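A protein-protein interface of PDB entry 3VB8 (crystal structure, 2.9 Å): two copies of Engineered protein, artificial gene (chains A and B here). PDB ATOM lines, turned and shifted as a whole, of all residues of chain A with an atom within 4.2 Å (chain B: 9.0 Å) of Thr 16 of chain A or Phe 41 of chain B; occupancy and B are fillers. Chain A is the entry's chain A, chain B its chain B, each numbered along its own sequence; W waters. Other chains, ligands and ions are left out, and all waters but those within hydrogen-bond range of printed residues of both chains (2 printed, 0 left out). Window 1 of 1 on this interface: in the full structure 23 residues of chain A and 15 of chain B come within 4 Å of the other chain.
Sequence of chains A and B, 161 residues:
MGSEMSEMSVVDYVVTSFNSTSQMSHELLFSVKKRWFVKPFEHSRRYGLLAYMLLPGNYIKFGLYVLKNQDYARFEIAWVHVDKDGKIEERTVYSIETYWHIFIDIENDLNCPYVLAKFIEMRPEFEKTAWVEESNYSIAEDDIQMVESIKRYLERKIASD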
ATOM      1  N   VAL A  15      -2.932   7.255  -9.996  1.00  0.00           N
ATOM      2  CA  VAL A  15      -3.271   6.396 -11.131  1.00  0.00           C
ATOM      3  C   VAL A  15      -3.843   7.232 -12.273  1.00  0.00           C
ATOM      4  O   VAL A  15      -4.285   8.353 -12.059  1.00  0.00           O
ATOM      5  CB  VAL A  15      -4.288   5.308 -10.731  1.00  0.00           C
ATOM      6  CG1 VAL A  15      -3.617   4.304  -9.746  1.00  0.00           C
ATOM      7  CG2 VAL A  15      -5.560   5.965 -10.146  1.00  0.00           C
ATOM      8  N   THR A  16      -3.830   6.709 -13.488  1.00  0.00           N
ATOM      9  CA  THR A  16      -4.350   7.505 -14.579  1.00  0.00           C
ATOM     10  C   THR A  16      -5.807   7.169 -14.753  1.00  0.00           C
ATOM     11  O   THR A  16      -6.196   6.003 -14.661  1.00  0.00           O
ATOM     12  CB  THR A  16      -3.611   7.232 -15.902  1.00  0.00           C
ATOM     13  OG1 THR A  16      -3.650   5.827 -16.181  1.00  0.00           O
ATOM     14  CG2 THR A  16      -2.159   7.712 -15.830  1.00  0.00           C
ATOM     15  N   SER A  17      -6.615   8.191 -14.998  1.00  0.00           N
ATOM     16  CA  SER A  17      -8.034   7.978 -15.202  1.00  0.00           C
ATOM     17  C   SER A  17      -8.515   9.056 -16.151  1.00  0.00           C
ATOM     18  O   SER A  17      -8.628  10.213 -15.757  1.00  0.00           O
ATOM     19  CB  SER A  17      -8.785   8.059 -13.857  1.00  0.00           C
ATOM     20  OG  SER A  17     -10.030   7.361 -13.883  1.00  0.00           O
ATOM     21  N   GLN A  23      -8.879   7.862 -27.144  1.00  0.00           N
ATOM     22  CA  GLN A  23      -8.412   6.870 -26.175  1.00  0.00           C
ATOM     23  C   GLN A  23      -9.016   6.955 -24.778  1.00  0.00           C
ATOM     24  O   GLN A  23      -9.781   7.856 -24.476  1.00  0.00           O
ATOM     25  CB  GLN A  23      -6.887   6.953 -26.049  1.00  0.00           C
ATOM     26  CG  GLN A  23      -6.361   8.352 -25.746  1.00  0.00           C
ATOM     27  CD  GLN A  23      -4.830   8.437 -25.789  1.00  0.00           C
ATOM     28  OE1 GLN A  23      -4.123   7.748 -25.041  1.00  0.00           O
ATOM     29  NE2 GLN A  23      -4.318   9.292 -26.669  1.00  0.00           N
ATOM     30  N   MET A  24      -8.653   6.010 -23.922  1.00  0.00           N
ATOM     31  CA  MET A  24      -9.144   6.007 -22.548  1.00  0.00           C
ATOM     32  C   MET A  24      -8.238   5.186 -21.627  1.00  0.00           C
ATOM     33  O   MET A  24      -7.784   4.118 -22.013  1.00  0.00           O
ATOM     34  CB  MET A  24     -10.564   5.437 -22.474  1.00  0.00           C
ATOM     35  CG  MET A  24     -11.124   5.464 -21.040  1.00  0.00           C
ATOM     36  SD  MET A  24     -12.581   4.445 -20.750  1.00  0.00           S
ATOM     37  CE  MET A  24     -11.763   2.884 -20.537  1.00  0.00           C
ATOM     38  N   SER A  25      -7.994   5.669 -20.411  1.00  0.00           N
ATOM     39  CA  SER A  25      -7.149   4.959 -19.453  1.00  0.00           C
ATOM     40  C   SER A  25      -7.885   4.902 -18.140  1.00  0.00           C
ATOM     41  O   SER A  25      -8.020   5.926 -17.470  1.00  0.00           O
ATOM     42  CB  SER A  25      -5.813   5.689 -19.245  1.00  0.00           C
ATOM     43  OG  SER A  25      -4.904   4.919 -18.468  1.00  0.00           O
ATOM     44  N   HIS A  26      -8.367   3.708 -17.799  1.00  0.00           N
ATOM     45  CA  HIS A  26      -9.094   3.454 -16.560  1.00  0.00           C
ATOM     46  C   HIS A  26      -8.265   2.591 -15.583  1.00  0.00           C
ATOM     47  O   HIS A  26      -7.989   1.408 -15.822  1.00  0.00           O
ATOM     48  CB  HIS A  26     -10.436   2.800 -16.921  1.00  0.00           C
ATOM     49  CG  HIS A  26     -11.365   2.619 -15.759  1.00  0.00           C
ATOM     50  ND1 HIS A  26     -11.454   3.531 -14.734  1.00  0.00           N
ATOM     51  CD2 HIS A  26     -12.236   1.629 -15.466  1.00  0.00           C
ATOM     52  CE1 HIS A  26     -12.342   3.109 -13.847  1.00  0.00           C
ATOM     53  NE2 HIS A  26     -12.831   1.957 -14.267  1.00  0.00           N
ATOM     54  N   GLU A  27      -7.844   3.217 -14.487  1.00  0.00           N
ATOM     55  CA  GLU A  27      -7.012   2.564 -13.469  1.00  0.00           C
ATOM     56  C   GLU A  27      -7.567   2.798 -12.064  1.00  0.00           C
ATOM     57  O   GLU A  27      -7.626   3.941 -11.589  1.00  0.00           O
ATOM     58  CB  GLU A  27      -5.604   3.150 -13.518  1.00  0.00           C
ATOM     59  CG  GLU A  27      -4.480   2.160 -13.647  1.00  0.00           C
ATOM     60  CD  GLU A  27      -3.216   2.844 -14.131  1.00  0.00           C
ATOM     61  OE1 GLU A  27      -2.764   3.808 -13.478  1.00  0.00           O
ATOM     62  OE2 GLU A  27      -2.679   2.422 -15.174  1.00  0.00           O
ATOM     63  N   GLY A  48      -6.136  14.087 -15.475  1.00  0.00           N
ATOM     64  CA  GLY A  48      -6.528  12.715 -15.739  1.00  0.00           C
ATOM     65  C   GLY A  48      -5.949  11.744 -14.732  1.00  0.00           C
ATOM     66  O   GLY A  48      -5.716  10.577 -15.046  1.00  0.00           O
ATOM     67  N   LEU A  49      -5.741  12.221 -13.513  1.00  0.00           N
ATOM     68  CA  LEU A  49      -5.188  11.393 -12.458  1.00  0.00           C
ATOM     69  C   LEU A  49      -6.097  11.219 -11.231  1.00  0.00           C
ATOM     70  O   LEU A  49      -6.999  12.008 -10.998  1.00  0.00           O
ATOM     71  CB  LEU A  49      -3.869  11.999 -11.993  1.00  0.00           C
ATOM     72  CG  LEU A  49      -2.814  12.416 -13.005  1.00  0.00           C
ATOM     73  CD1 LEU A  49      -1.774  13.249 -12.256  1.00  0.00           C
ATOM     74  CD2 LEU A  49      -2.188  11.180 -13.664  1.00  0.00           C
ATOM     75  N   TYR A  65      -7.091  -0.079 -20.689  1.00  0.00           N
ATOM     76  CA  TYR A  65      -6.477   0.939 -21.534  1.00  0.00           C
ATOM     77  C   TYR A  65      -7.047   0.745 -22.916  1.00  0.00           C
ATOM     78  O   TYR A  65      -6.866  -0.327 -23.493  1.00  0.00           O
ATOM     79  CB  TYR A  65      -4.963   0.743 -21.563  1.00  0.00           C
ATOM     80  CG  TYR A  65      -4.370   0.567 -20.180  1.00  0.00           C
ATOM     81  CD1 TYR A  65      -4.196   1.656 -19.322  1.00  0.00           C
ATOM     82  CD2 TYR A  65      -4.060  -0.701 -19.692  1.00  0.00           C
ATOM     83  CE1 TYR A  65      -3.736   1.482 -18.007  1.00  0.00           C
ATOM     84  CE2 TYR A  65      -3.603  -0.876 -18.389  1.00  0.00           C
ATOM     85  CZ  TYR A  65      -3.447   0.214 -17.552  1.00  0.00           C
ATOM     86  OH  TYR A  65      -3.035   0.024 -16.254  1.00  0.00           O
ATOM     87  N   VAL A  66      -7.715   1.754 -23.465  1.00  0.00           N
ATOM     88  CA  VAL A  66      -8.322   1.591 -24.782  1.00  0.00           C
ATOM     89  C   VAL A  66      -7.972   2.627 -25.862  1.00  0.00           C
ATOM     90  O   VAL A  66      -7.871   3.813 -25.595  1.00  0.00           O
ATOM     91  CB  VAL A  66      -9.860   1.560 -24.643  1.00  0.00           C
ATOM     92  CG1 VAL A  66     -10.502   1.600 -26.012  1.00  0.00           C
ATOM     93  CG2 VAL A  66     -10.265   0.298 -23.902  1.00  0.00           C
ATOM     94  N   LEU A  67      -7.812   2.145 -27.091  1.00  0.00           N
ATOM     95  CA  LEU A  67      -7.541   2.972 -28.270  1.00  0.00           C
ATOM     96  C   LEU A  67      -8.914   2.850 -28.908  1.00  0.00           C
ATOM     97  O   LEU A  67      -9.167   1.916 -29.652  1.00  0.00           O
ATOM     98  CB  LEU A  67      -6.451   2.333 -29.160  1.00  0.00           C
ATOM     99  CG  LEU A  67      -4.947   2.550 -28.984  1.00  0.00           C
ATOM    100  CD1 LEU A  67      -4.661   4.030 -29.098  1.00  0.00           C
ATOM    101  CD2 LEU A  67      -4.500   2.021 -27.642  1.00  0.00           C
ATOM    102  N   VAL B  10      -0.077  -2.895 -32.027  1.00  0.00           N
ATOM    103  CA  VAL B  10      -0.022  -1.989 -30.877  1.00  0.00           C
ATOM    104  C   VAL B  10       1.185  -2.372 -30.036  1.00  0.00           C
ATOM    105  O   VAL B  10       1.219  -3.463 -29.455  1.00  0.00           O
ATOM    106  CB  VAL B  10      -1.247  -2.141 -29.997  1.00  0.00           C
ATOM    107  CG1 VAL B  10      -2.422  -1.407 -30.601  1.00  0.00           C
ATOM    108  CG2 VAL B  10      -1.582  -3.622 -29.849  1.00  0.00           C
ATOM    109  N   VAL B  11       2.181  -1.493 -29.982  1.00  0.00           N
ATOM    110  CA  VAL B  11       3.390  -1.791 -29.216  1.00  0.00           C
ATOM    111  C   VAL B  11       3.660  -0.905 -27.997  1.00  0.00           C
ATOM    112  O   VAL B  11       3.619   0.329 -28.067  1.00  0.00           O
ATOM    113  CB  VAL B  11       4.635  -1.741 -30.106  1.00  0.00           C
ATOM    114  CG1 VAL B  11       4.622  -2.907 -31.054  1.00  0.00           C
ATOM    115  CG2 VAL B  11       4.640  -0.479 -30.900  1.00  0.00           C
ATOM    116  N   ASP B  12       3.952  -1.547 -26.872  1.00  0.00           N
ATOM    117  CA  ASP B  12       4.259  -0.820 -25.649  1.00  0.00           C
ATOM    118  C   ASP B  12       5.548  -0.045 -25.830  1.00  0.00           C
ATOM    119  O   ASP B  12       6.541  -0.574 -26.319  1.00  0.00           O
ATOM    120  CB  ASP B  12       4.402  -1.784 -24.473  1.00  0.00           C
ATOM    121  CG  ASP B  12       3.076  -2.218 -23.914  1.00  0.00           C
ATOM    122  OD1 ASP B  12       2.398  -1.371 -23.296  1.00  0.00           O
ATOM    123  OD2 ASP B  12       2.720  -3.402 -24.086  1.00  0.00           O
ATOM    124  N   TYR B  13       5.523   1.221 -25.444  1.00  0.00           N
ATOM    125  CA  TYR B  13       6.696   2.054 -25.536  1.00  0.00           C
ATOM    126  C   TYR B  13       6.702   2.842 -24.248  1.00  0.00           C
ATOM    127  O   TYR B  13       5.712   3.502 -23.918  1.00  0.00           O
ATOM    128  CB  TYR B  13       6.622   2.992 -26.729  1.00  0.00           C
ATOM    129  CG  TYR B  13       7.919   3.732 -26.937  1.00  0.00           C
ATOM    130  CD1 TYR B  13       8.956   3.177 -27.697  1.00  0.00           C
ATOM    131  CD2 TYR B  13       8.126   4.983 -26.366  1.00  0.00           C
ATOM    132  CE1 TYR B  13      10.176   3.864 -27.888  1.00  0.00           C
ATOM    133  CE2 TYR B  13       9.329   5.672 -26.549  1.00  0.00           C
ATOM    134  CZ  TYR B  13      10.346   5.116 -27.309  1.00  0.00           C
ATOM    135  OH  TYR B  13      11.497   5.854 -27.494  1.00  0.00           O
ATOM    136  N   VAL B  38       2.000  12.811 -27.670  1.00  0.00           N
ATOM    137  CA  VAL B  38       1.190  11.630 -27.476  1.00  0.00           C
ATOM    138  C   VAL B  38       0.711  11.617 -26.047  1.00  0.00           C
ATOM    139  O   VAL B  38       1.325  12.256 -25.204  1.00  0.00           O
ATOM    140  CB  VAL B  38       2.032  10.401 -27.755  1.00  0.00           C
ATOM    141  CG1 VAL B  38       1.167   9.140 -27.831  1.00  0.00           C
ATOM    142  CG2 VAL B  38       2.794  10.631 -29.037  1.00  0.00           C
ATOM    143  N   LYS B  39      -0.388  10.911 -25.787  1.00  0.00           N
ATOM    144  CA  LYS B  39      -0.972  10.802 -24.448  1.00  0.00           C
ATOM    145  C   LYS B  39      -0.587   9.479 -23.740  1.00  0.00           C
ATOM    146  O   LYS B  39      -0.848   8.387 -24.244  1.00  0.00           O
ATOM    147  CB  LYS B  39      -2.493  10.912 -24.562  1.00  0.00           C
ATOM    148  CG  LYS B  39      -3.218  11.291 -23.288  1.00  0.00           C
ATOM    149  CD  LYS B  39      -2.823  12.686 -22.820  1.00  0.00           C
ATOM    150  CE  LYS B  39      -3.774  13.264 -21.767  1.00  0.00           C
ATOM    151  NZ  LYS B  39      -4.043  12.377 -20.601  1.00  0.00           N
ATOM    152  N   PRO B  40       0.031   9.569 -22.549  1.00  0.00           N
ATOM    153  CA  PRO B  40       0.435   8.372 -21.802  1.00  0.00           C
ATOM    154  C   PRO B  40      -0.759   7.601 -21.277  1.00  0.00           C
ATOM    155  O   PRO B  40      -1.799   8.189 -21.015  1.00  0.00           O
ATOM    156  CB  PRO B  40       1.286   8.939 -20.663  1.00  0.00           C
ATOM    157  CG  PRO B  40       1.792  10.213 -21.206  1.00  0.00           C
ATOM    158  CD  PRO B  40       0.580  10.777 -21.918  1.00  0.00           C
ATOM    159  N   PHE B  41      -0.602   6.289 -21.129  1.00  0.00           N
ATOM    160  CA  PHE B  41      -1.652   5.424 -20.609  1.00  0.00           C
ATOM    161  C   PHE B  41      -1.325   5.104 -19.153  1.00  0.00           C
ATOM    162  O   PHE B  41      -2.129   4.494 -18.446  1.00  0.00           O
ATOM    163  CB  PHE B  41      -1.716   4.125 -21.416  1.00  0.00           C
ATOM    164  CG  PHE B  41      -2.479   4.246 -22.697  1.00  0.00           C
ATOM    165  CD1 PHE B  41      -3.860   4.072 -22.714  1.00  0.00           C
ATOM    166  CD2 PHE B  41      -1.832   4.597 -23.879  1.00  0.00           C
ATOM    167  CE1 PHE B  41      -4.592   4.253 -23.891  1.00  0.00           C
ATOM    168  CE2 PHE B  41      -2.552   4.781 -25.064  1.00  0.00           C
ATOM    169  CZ  PHE B  41      -3.934   4.612 -25.071  1.00  0.00           C
ATOM    170  N   GLU B  42      -0.120   5.489 -18.729  1.00  0.00           N
ATOM    171  CA  GLU B  42       0.341   5.251 -17.362  1.00  0.00           C
ATOM    172  C   GLU B  42       1.415   6.249 -16.949  1.00  0.00           C
ATOM    173  O   GLU B  42       2.259   6.621 -17.753  1.00  0.00           O
ATOM    174  CB  GLU B  42       0.903   3.826 -17.214  1.00  0.00           C
ATOM    175  CG  GLU B  42      -0.137   2.719 -17.307  1.00  0.00           C
ATOM    176  CD  GLU B  42       0.497   1.340 -17.389  1.00  0.00           C
ATOM    177  OE1 GLU B  42       1.203   1.086 -18.388  1.00  0.00           O
ATOM    178  OE2 GLU B  42       0.303   0.509 -16.469  1.00  0.00           O
ATOM    179  N   HIS B  43       1.357   6.685 -15.695  1.00  0.00           N
ATOM    180  CA  HIS B  43       2.326   7.620 -15.133  1.00  0.00           C
ATOM    181  C   HIS B  43       2.785   7.052 -13.794  1.00  0.00           C
ATOM    182  O   HIS B  43       2.087   7.178 -12.787  1.00  0.00           O
ATOM    183  CB  HIS B  43       1.701   8.996 -14.865  1.00  0.00           C
ATOM    184  CG  HIS B  43       1.194   9.703 -16.092  1.00  0.00           C
ATOM    185  ND1 HIS B  43       0.070   9.295 -16.770  1.00  0.00           N
ATOM    186  CD2 HIS B  43       1.651  10.796 -16.747  1.00  0.00           C
ATOM    187  CE1 HIS B  43      -0.148  10.099 -17.798  1.00  0.00           C
ATOM    188  NE2 HIS B  43       0.799  11.017 -17.807  1.00  0.00           N
ATOM    189  N   SER B  44       3.948   6.418 -13.771  1.00  0.00           N
ATOM    190  CA  SER B  44       4.427   5.866 -12.521  1.00  0.00           C
ATOM    191  C   SER B  44       5.712   6.548 -12.038  1.00  0.00           C
ATOM    192  O   SER B  44       6.809   6.192 -12.468  1.00  0.00           O
ATOM    193  CB  SER B  44       4.667   4.372 -12.677  1.00  0.00           C
ATOM    194  OG  SER B  44       4.951   3.796 -11.423  1.00  0.00           O
ATOM    195  N   ARG B  45       5.566   7.513 -11.132  1.00  0.00           N
ATOM    196  CA  ARG B  45       6.702   8.247 -10.579  1.00  0.00           C
ATOM    197  C   ARG B  45       7.413   7.308  -9.639  1.00  0.00           C
ATOM    198  O   ARG B  45       8.537   7.542  -9.215  1.00  0.00           O
ATOM    199  CB  ARG B  45       6.229   9.510  -9.835  1.00  0.00           C
ATOM    200  CG  ARG B  45       5.089   9.279  -8.853  1.00  0.00           C
ATOM    201  CD  ARG B  45       3.787   9.054  -9.612  1.00  0.00           C
ATOM    202  NE  ARG B  45       3.470  10.170 -10.504  1.00  0.00           N
ATOM    203  CZ  ARG B  45       3.087  11.376 -10.093  1.00  0.00           C
ATOM    204  NH1 ARG B  45       2.966  11.639  -8.796  1.00  0.00           N
ATOM    205  NH2 ARG B  45       2.826  12.326 -10.979  1.00  0.00           N
ATOM    206  N   LEU B  49       8.744   6.602 -14.741  1.00  0.00           N
ATOM    207  CA  LEU B  49       8.474   6.403 -16.153  1.00  0.00           C
ATOM    208  C   LEU B  49       7.056   6.731 -16.597  1.00  0.00           C
ATOM    209  O   LEU B  49       6.159   6.862 -15.776  1.00  0.00           O
ATOM    210  CB  LEU B  49       8.822   4.966 -16.535  1.00  0.00           C
ATOM    211  CG  LEU B  49       8.061   3.801 -15.924  1.00  0.00           C
ATOM    212  CD1 LEU B  49       6.694   3.672 -16.556  1.00  0.00           C
ATOM    213  CD2 LEU B  49       8.833   2.522 -16.202  1.00  0.00           C
ATOM    214  N   LEU B  50       6.883   6.851 -17.913  1.00  0.00           N
ATOM    215  CA  LEU B  50       5.601   7.160 -18.539  1.00  0.00           C
ATOM    216  C   LEU B  50       5.501   6.077 -19.564  1.00  0.00           C
ATOM    217  O   LEU B  50       6.489   5.790 -20.225  1.00  0.00           O
ATOM    218  CB  LEU B  50       5.652   8.511 -19.255  1.00  0.00           C
ATOM    219  CG  LEU B  50       5.941   9.816 -18.509  1.00  0.00           C
ATOM    220  CD1 LEU B  50       6.062  10.958 -19.508  1.00  0.00           C
ATOM    221  CD2 LEU B  50       4.835  10.078 -17.496  1.00  0.00           C
ATOM    222  N   ALA B  51       4.334   5.468 -19.699  1.00  0.00           N
ATOM    223  CA  ALA B  51       4.184   4.392 -20.663  1.00  0.00           C
ATOM    224  C   ALA B  51       3.091   4.676 -21.686  1.00  0.00           C
ATOM    225  O   ALA B  51       2.013   5.138 -21.334  1.00  0.00           O
ATOM    226  CB  ALA B  51       3.894   3.108 -19.933  1.00  0.00           C
ATOM    227  N   TYR B  52       3.381   4.388 -22.950  1.00  0.00           N
ATOM    228  CA  TYR B  52       2.432   4.601 -24.041  1.00  0.00           C
ATOM    229  C   TYR B  52       1.988   3.270 -24.678  1.00  0.00           C
ATOM    230  O   TYR B  52       2.346   2.177 -24.217  1.00  0.00           O
ATOM    231  CB  TYR B  52       3.077   5.464 -25.130  1.00  0.00           C
ATOM    232  CG  TYR B  52       3.702   6.757 -24.668  1.00  0.00           C
ATOM    233  CD1 TYR B  52       2.963   7.923 -24.598  1.00  0.00           C
ATOM    234  CD2 TYR B  52       5.059   6.821 -24.360  1.00  0.00           C
ATOM    235  CE1 TYR B  52       3.566   9.126 -24.233  1.00  0.00           C
ATOM    236  CE2 TYR B  52       5.666   8.012 -23.996  1.00  0.00           C
ATOM    237  CZ  TYR B  52       4.924   9.159 -23.936  1.00  0.00           C
ATOM    238  OH  TYR B  52       5.567  10.333 -23.599  1.00  0.00           O
ATOM    239  N   MET B  53       1.211   3.402 -25.751  1.00  0.00           N
ATOM    240  CA  MET B  53       0.703   2.291 -26.553  1.00  0.00           C
ATOM    241  C   MET B  53       0.673   2.863 -27.959  1.00  0.00           C
ATOM    242  O   MET B  53      -0.192   3.678 -28.288  1.00  0.00           O
ATOM    243  CB  MET B  53      -0.702   1.868 -26.118  1.00  0.00           C
ATOM    244  CG  MET B  53      -0.770   1.150 -24.789  1.00  0.00           C
ATOM    245  SD  MET B  53      -2.034  -0.128 -24.790  1.00  0.00           S
ATOM    246  CE  MET B  53      -3.514   0.797 -24.509  1.00  0.00           C
ATOM    247  N   LEU B  54       1.649   2.471 -28.769  1.00  0.00           N
ATOM    248  CA  LEU B  54       1.732   2.995 -30.116  1.00  0.00           C
ATOM    249  C   LEU B  54       1.164   2.114 -31.247  1.00  0.00           C
ATOM    250  O   LEU B  54       1.066   0.887 -31.144  1.00  0.00           O
ATOM    251  CB  LEU B  54       3.184   3.346 -30.446  1.00  0.00           C
ATOM    252  CG  LEU B  54       4.004   4.240 -29.520  1.00  0.00           C
ATOM    253  CD1 LEU B  54       5.254   4.709 -30.241  1.00  0.00           C
ATOM    254  CD2 LEU B  54       3.216   5.435 -29.139  1.00  0.00           C
ATOM    255  N   LEU B  55       0.807   2.781 -32.339  1.00  0.00           N
ATOM    256  CA  LEU B  55       0.266   2.152 -33.529  1.00  0.00           C
ATOM    257  C   LEU B  55       1.308   2.494 -34.554  1.00  0.00           C
ATOM    258  O   LEU B  55       1.983   3.489 -34.409  1.00  0.00           O
ATOM    259  CB  LEU B  55      -1.071   2.800 -33.882  1.00  0.00           C
ATOM    260  CG  LEU B  55      -2.258   2.582 -32.931  1.00  0.00           C
ATOM    261  CD1 LEU B  55      -3.275   3.703 -33.159  1.00  0.00           C
ATOM    262  CD2 LEU B  55      -2.860   1.172 -33.130  1.00  0.00           C
ATOM    263  N   THR B 129       5.799  12.913 -12.357  1.00  0.00           N
ATOM    264  CA  THR B 129       6.145  12.519 -13.723  1.00  0.00           C
ATOM    265  C   THR B 129       5.497  13.523 -14.613  1.00  0.00           C
ATOM    266  O   THR B 129       4.523  14.145 -14.213  1.00  0.00           O
ATOM    267  CB  THR B 129       5.590  11.112 -14.116  1.00  0.00           C
ATOM    268  OG1 THR B 129       4.186  11.035 -13.820  1.00  0.00           O
ATOM    269  CG2 THR B 129       6.348  10.010 -13.398  1.00  0.00           C
ATOM    270  N   ALA B 130       6.023  13.674 -15.817  1.00  0.00           N
ATOM    271  CA  ALA B 130       5.457  14.635 -16.731  1.00  0.00           C
ATOM    272  C   ALA B 130       3.995  14.298 -16.998  1.00  0.00           C
ATOM    273  O   ALA B 130       3.624  13.133 -16.939  1.00  0.00           O
ATOM    274  CB  ALA B 130       6.257  14.637 -18.019  1.00  0.00           C
ATOM    275  N   TRP B 131       3.174  15.315 -17.267  1.00  0.00           N
ATOM    276  CA  TRP B 131       1.751  15.124 -17.565  1.00  0.00           C
ATOM    277  C   TRP B 131       1.349  15.835 -18.872  1.00  0.00           C
ATOM    278  O   TRP B 131       1.304  17.061 -18.928  1.00  0.00           O
ATOM    279  CB  TRP B 131       0.891  15.661 -16.417  1.00  0.00           C
ATOM    280  CG  TRP B 131       1.128  15.029 -15.113  1.00  0.00           C
ATOM    281  CD1 TRP B 131       1.295  13.703 -14.869  1.00  0.00           C
ATOM    282  CD2 TRP B 131       1.150  15.679 -13.836  1.00  0.00           C
ATOM    283  NE1 TRP B 131       1.420  13.473 -13.515  1.00  0.00           N
ATOM    284  CE2 TRP B 131       1.334  14.674 -12.856  1.00  0.00           C
ATOM    285  CE3 TRP B 131       1.030  17.013 -13.421  1.00  0.00           C
ATOM    286  CZ2 TRP B 131       1.402  14.970 -11.482  1.00  0.00           C
ATOM    287  CZ3 TRP B 131       1.097  17.303 -12.062  1.00  0.00           C
ATOM    288  CH2 TRP B 131       1.280  16.287 -11.109  1.00  0.00           C
ATOM    289  N   VAL B 132       1.076  15.081 -19.932  1.00  0.00           N
ATOM    290  CA  VAL B 132       0.690  15.718 -21.191  1.00  0.00           C
ATOM    291  C   VAL B 132      -0.739  16.220 -21.114  1.00  0.00           C
ATOM    292  O   VAL B 132      -1.647  15.457 -20.783  1.00  0.00           O
ATOM    293  CB  VAL B 132       0.788  14.748 -22.356  1.00  0.00           C
ATOM    294  CG1 VAL B 132       0.425  15.451 -23.649  1.00  0.00           C
ATOM    295  CG2 VAL B 132       2.187  14.160 -22.412  1.00  0.00           C
HETATM  296  O   HOH W   1      -4.003   6.853 -22.154  1.00  0.00           O
HETATM  297  O   HOH W   2      -0.237   5.211 -13.904  1.00  0.00           O
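The backbone carbonyl oxygen (O) of Phe 41 of chain B lies within hydrogen-bond range of the side-chain hydroxyl (OG1) of Thr 16 of chain A, 3.0 Å away. The side-chain amide oxygen (OE1) of Gln 23 of chain A sits close to the backbone carbonyl oxygen (O) of Lys 39 of chain B (3.4 Å). The side-chain hydroxyl of Tyr 65 of chain A lies within hydrogen-bond range of the side-chain carboxylate of Glu 42 of chain B. The side-chain hydroxyl (OG) of Ser 25 of chain A is in hydrogen-bond range of the backbone carbonyl oxygen (O) of Phe 41 of chain B, at 2.8 Å.
N of Thr 16 of chain A lies within hydrogen-bond range of OE1 of Glu 27 of chain A (3.1 Å). OE2 of Glu 27 of chain A sits at hydrogen-bond distance from OH of Tyr 65 of chain A (2.7 Å). The backbone carbonyl oxygen (O) of Met 24 of chain A lies within hydrogen-bond range of the backbone NH (N) of Val 66 of chain A (2.8 Å). The side-chain hydroxyl (OG) of Ser 25 of chain A lies within hydrogen-bond range of the side-chain hydroxyl (OG1) of Thr 16 of chain A, at 2.8 Å. The backbone carbonyl oxygen (O) of Thr 129 of chain B sits at hydrogen-bond distance from the indole nitrogen (NE1) of Trp 131 of chain B. The backbone carbonyl oxygen (O) of Ala 51 of chain B is in hydrogen-bond range of the backbone NH (N) of Phe 41 of chain B, at 2.9 Å.
Thr 16 of chain A touches Glu 42 of chain B. ND1 of His 43 of chain B touches CG2 of Thr 16 of chain A (2.9 Å). Gln 23 of chain A touches Phe 41 of chain B (OE1 to CZ, 3.1 Å). Phe 41 of chain B touches Met 24 of chain A. Glu 27 of chain A touches Phe 41 of chain B. Glu 27 of chain A touches Glu 42 of chain B. Phe 41 of chain B touches Tyr 65 of chain A. Tyr 65 of chain A touches Met 53 of chain B (CB to CE, 3.3 Å). Val 66 of chain A touches Phe 41 of chain B (O to CE1, 3.7 Å). Phe 41 of chain B touches Leu 67 of chain A (CZ to CD2, 3.7 Å).
No residue of chain B comes within 4 Å of Val 15 of chain A. No residue of chain B comes within 4 Å of Ser 17 of chain A. Printed residues of chain B within 4 Å of Gln 23 of chain A: Lys 39 (3.2 Å) and Phe 41 (3.1 Å). Of chain B, only Phe 41 and Glu 42 come within 4 Å of Glu 27 of chain A. Of the printed residues of chain B, Leu 49 of chain A touches Trp 131. Printed residues of chain B within 4 Å of Val 66 of chain A: Phe 41 (3.7 Å). Printed residues of chain B within 4 Å of Leu 67 of chain A: Phe 41 and Met 53. Printed residues of chain A within 4 Å of Met 53 of chain B: Tyr 65 (3.3 Å) and Leu 67 (3.5 Å). Leu 55 of chain B touches none of the printed residues of chain A. The nearest residue of chain B that does not touch Thr 16 of chain A is Pro 40 of chain B (5.2 Å).
Of the 13 printed residues of chain A, 9 touch a printed residue of chain B. Along chain A the printed residues that touch a printed residue of chain B span positions 16 to 67. Hydrophobic or aromatic side chains of chain B within 4 Å of the printed part of chain A: Phe 41, His 43, Met 53 and Trp 131.
Position printed for both chains: 49. Of the 16 pairs that touch across the chains among the printed residues, none has its exchanged pair printed and touching as well.
Water W2 lies within hydrogen-bond range of N of His 43 of chain B (2.8 Å) and OE1 of Glu 27 of chain A (2.9 Å). Water W1 lies within hydrogen-bond range of the backbone carbonyl oxygen of Pro 40 of chain B (2.8 Å) and the side-chain amide oxygen of Gln 23 of chain A (3.0 Å).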
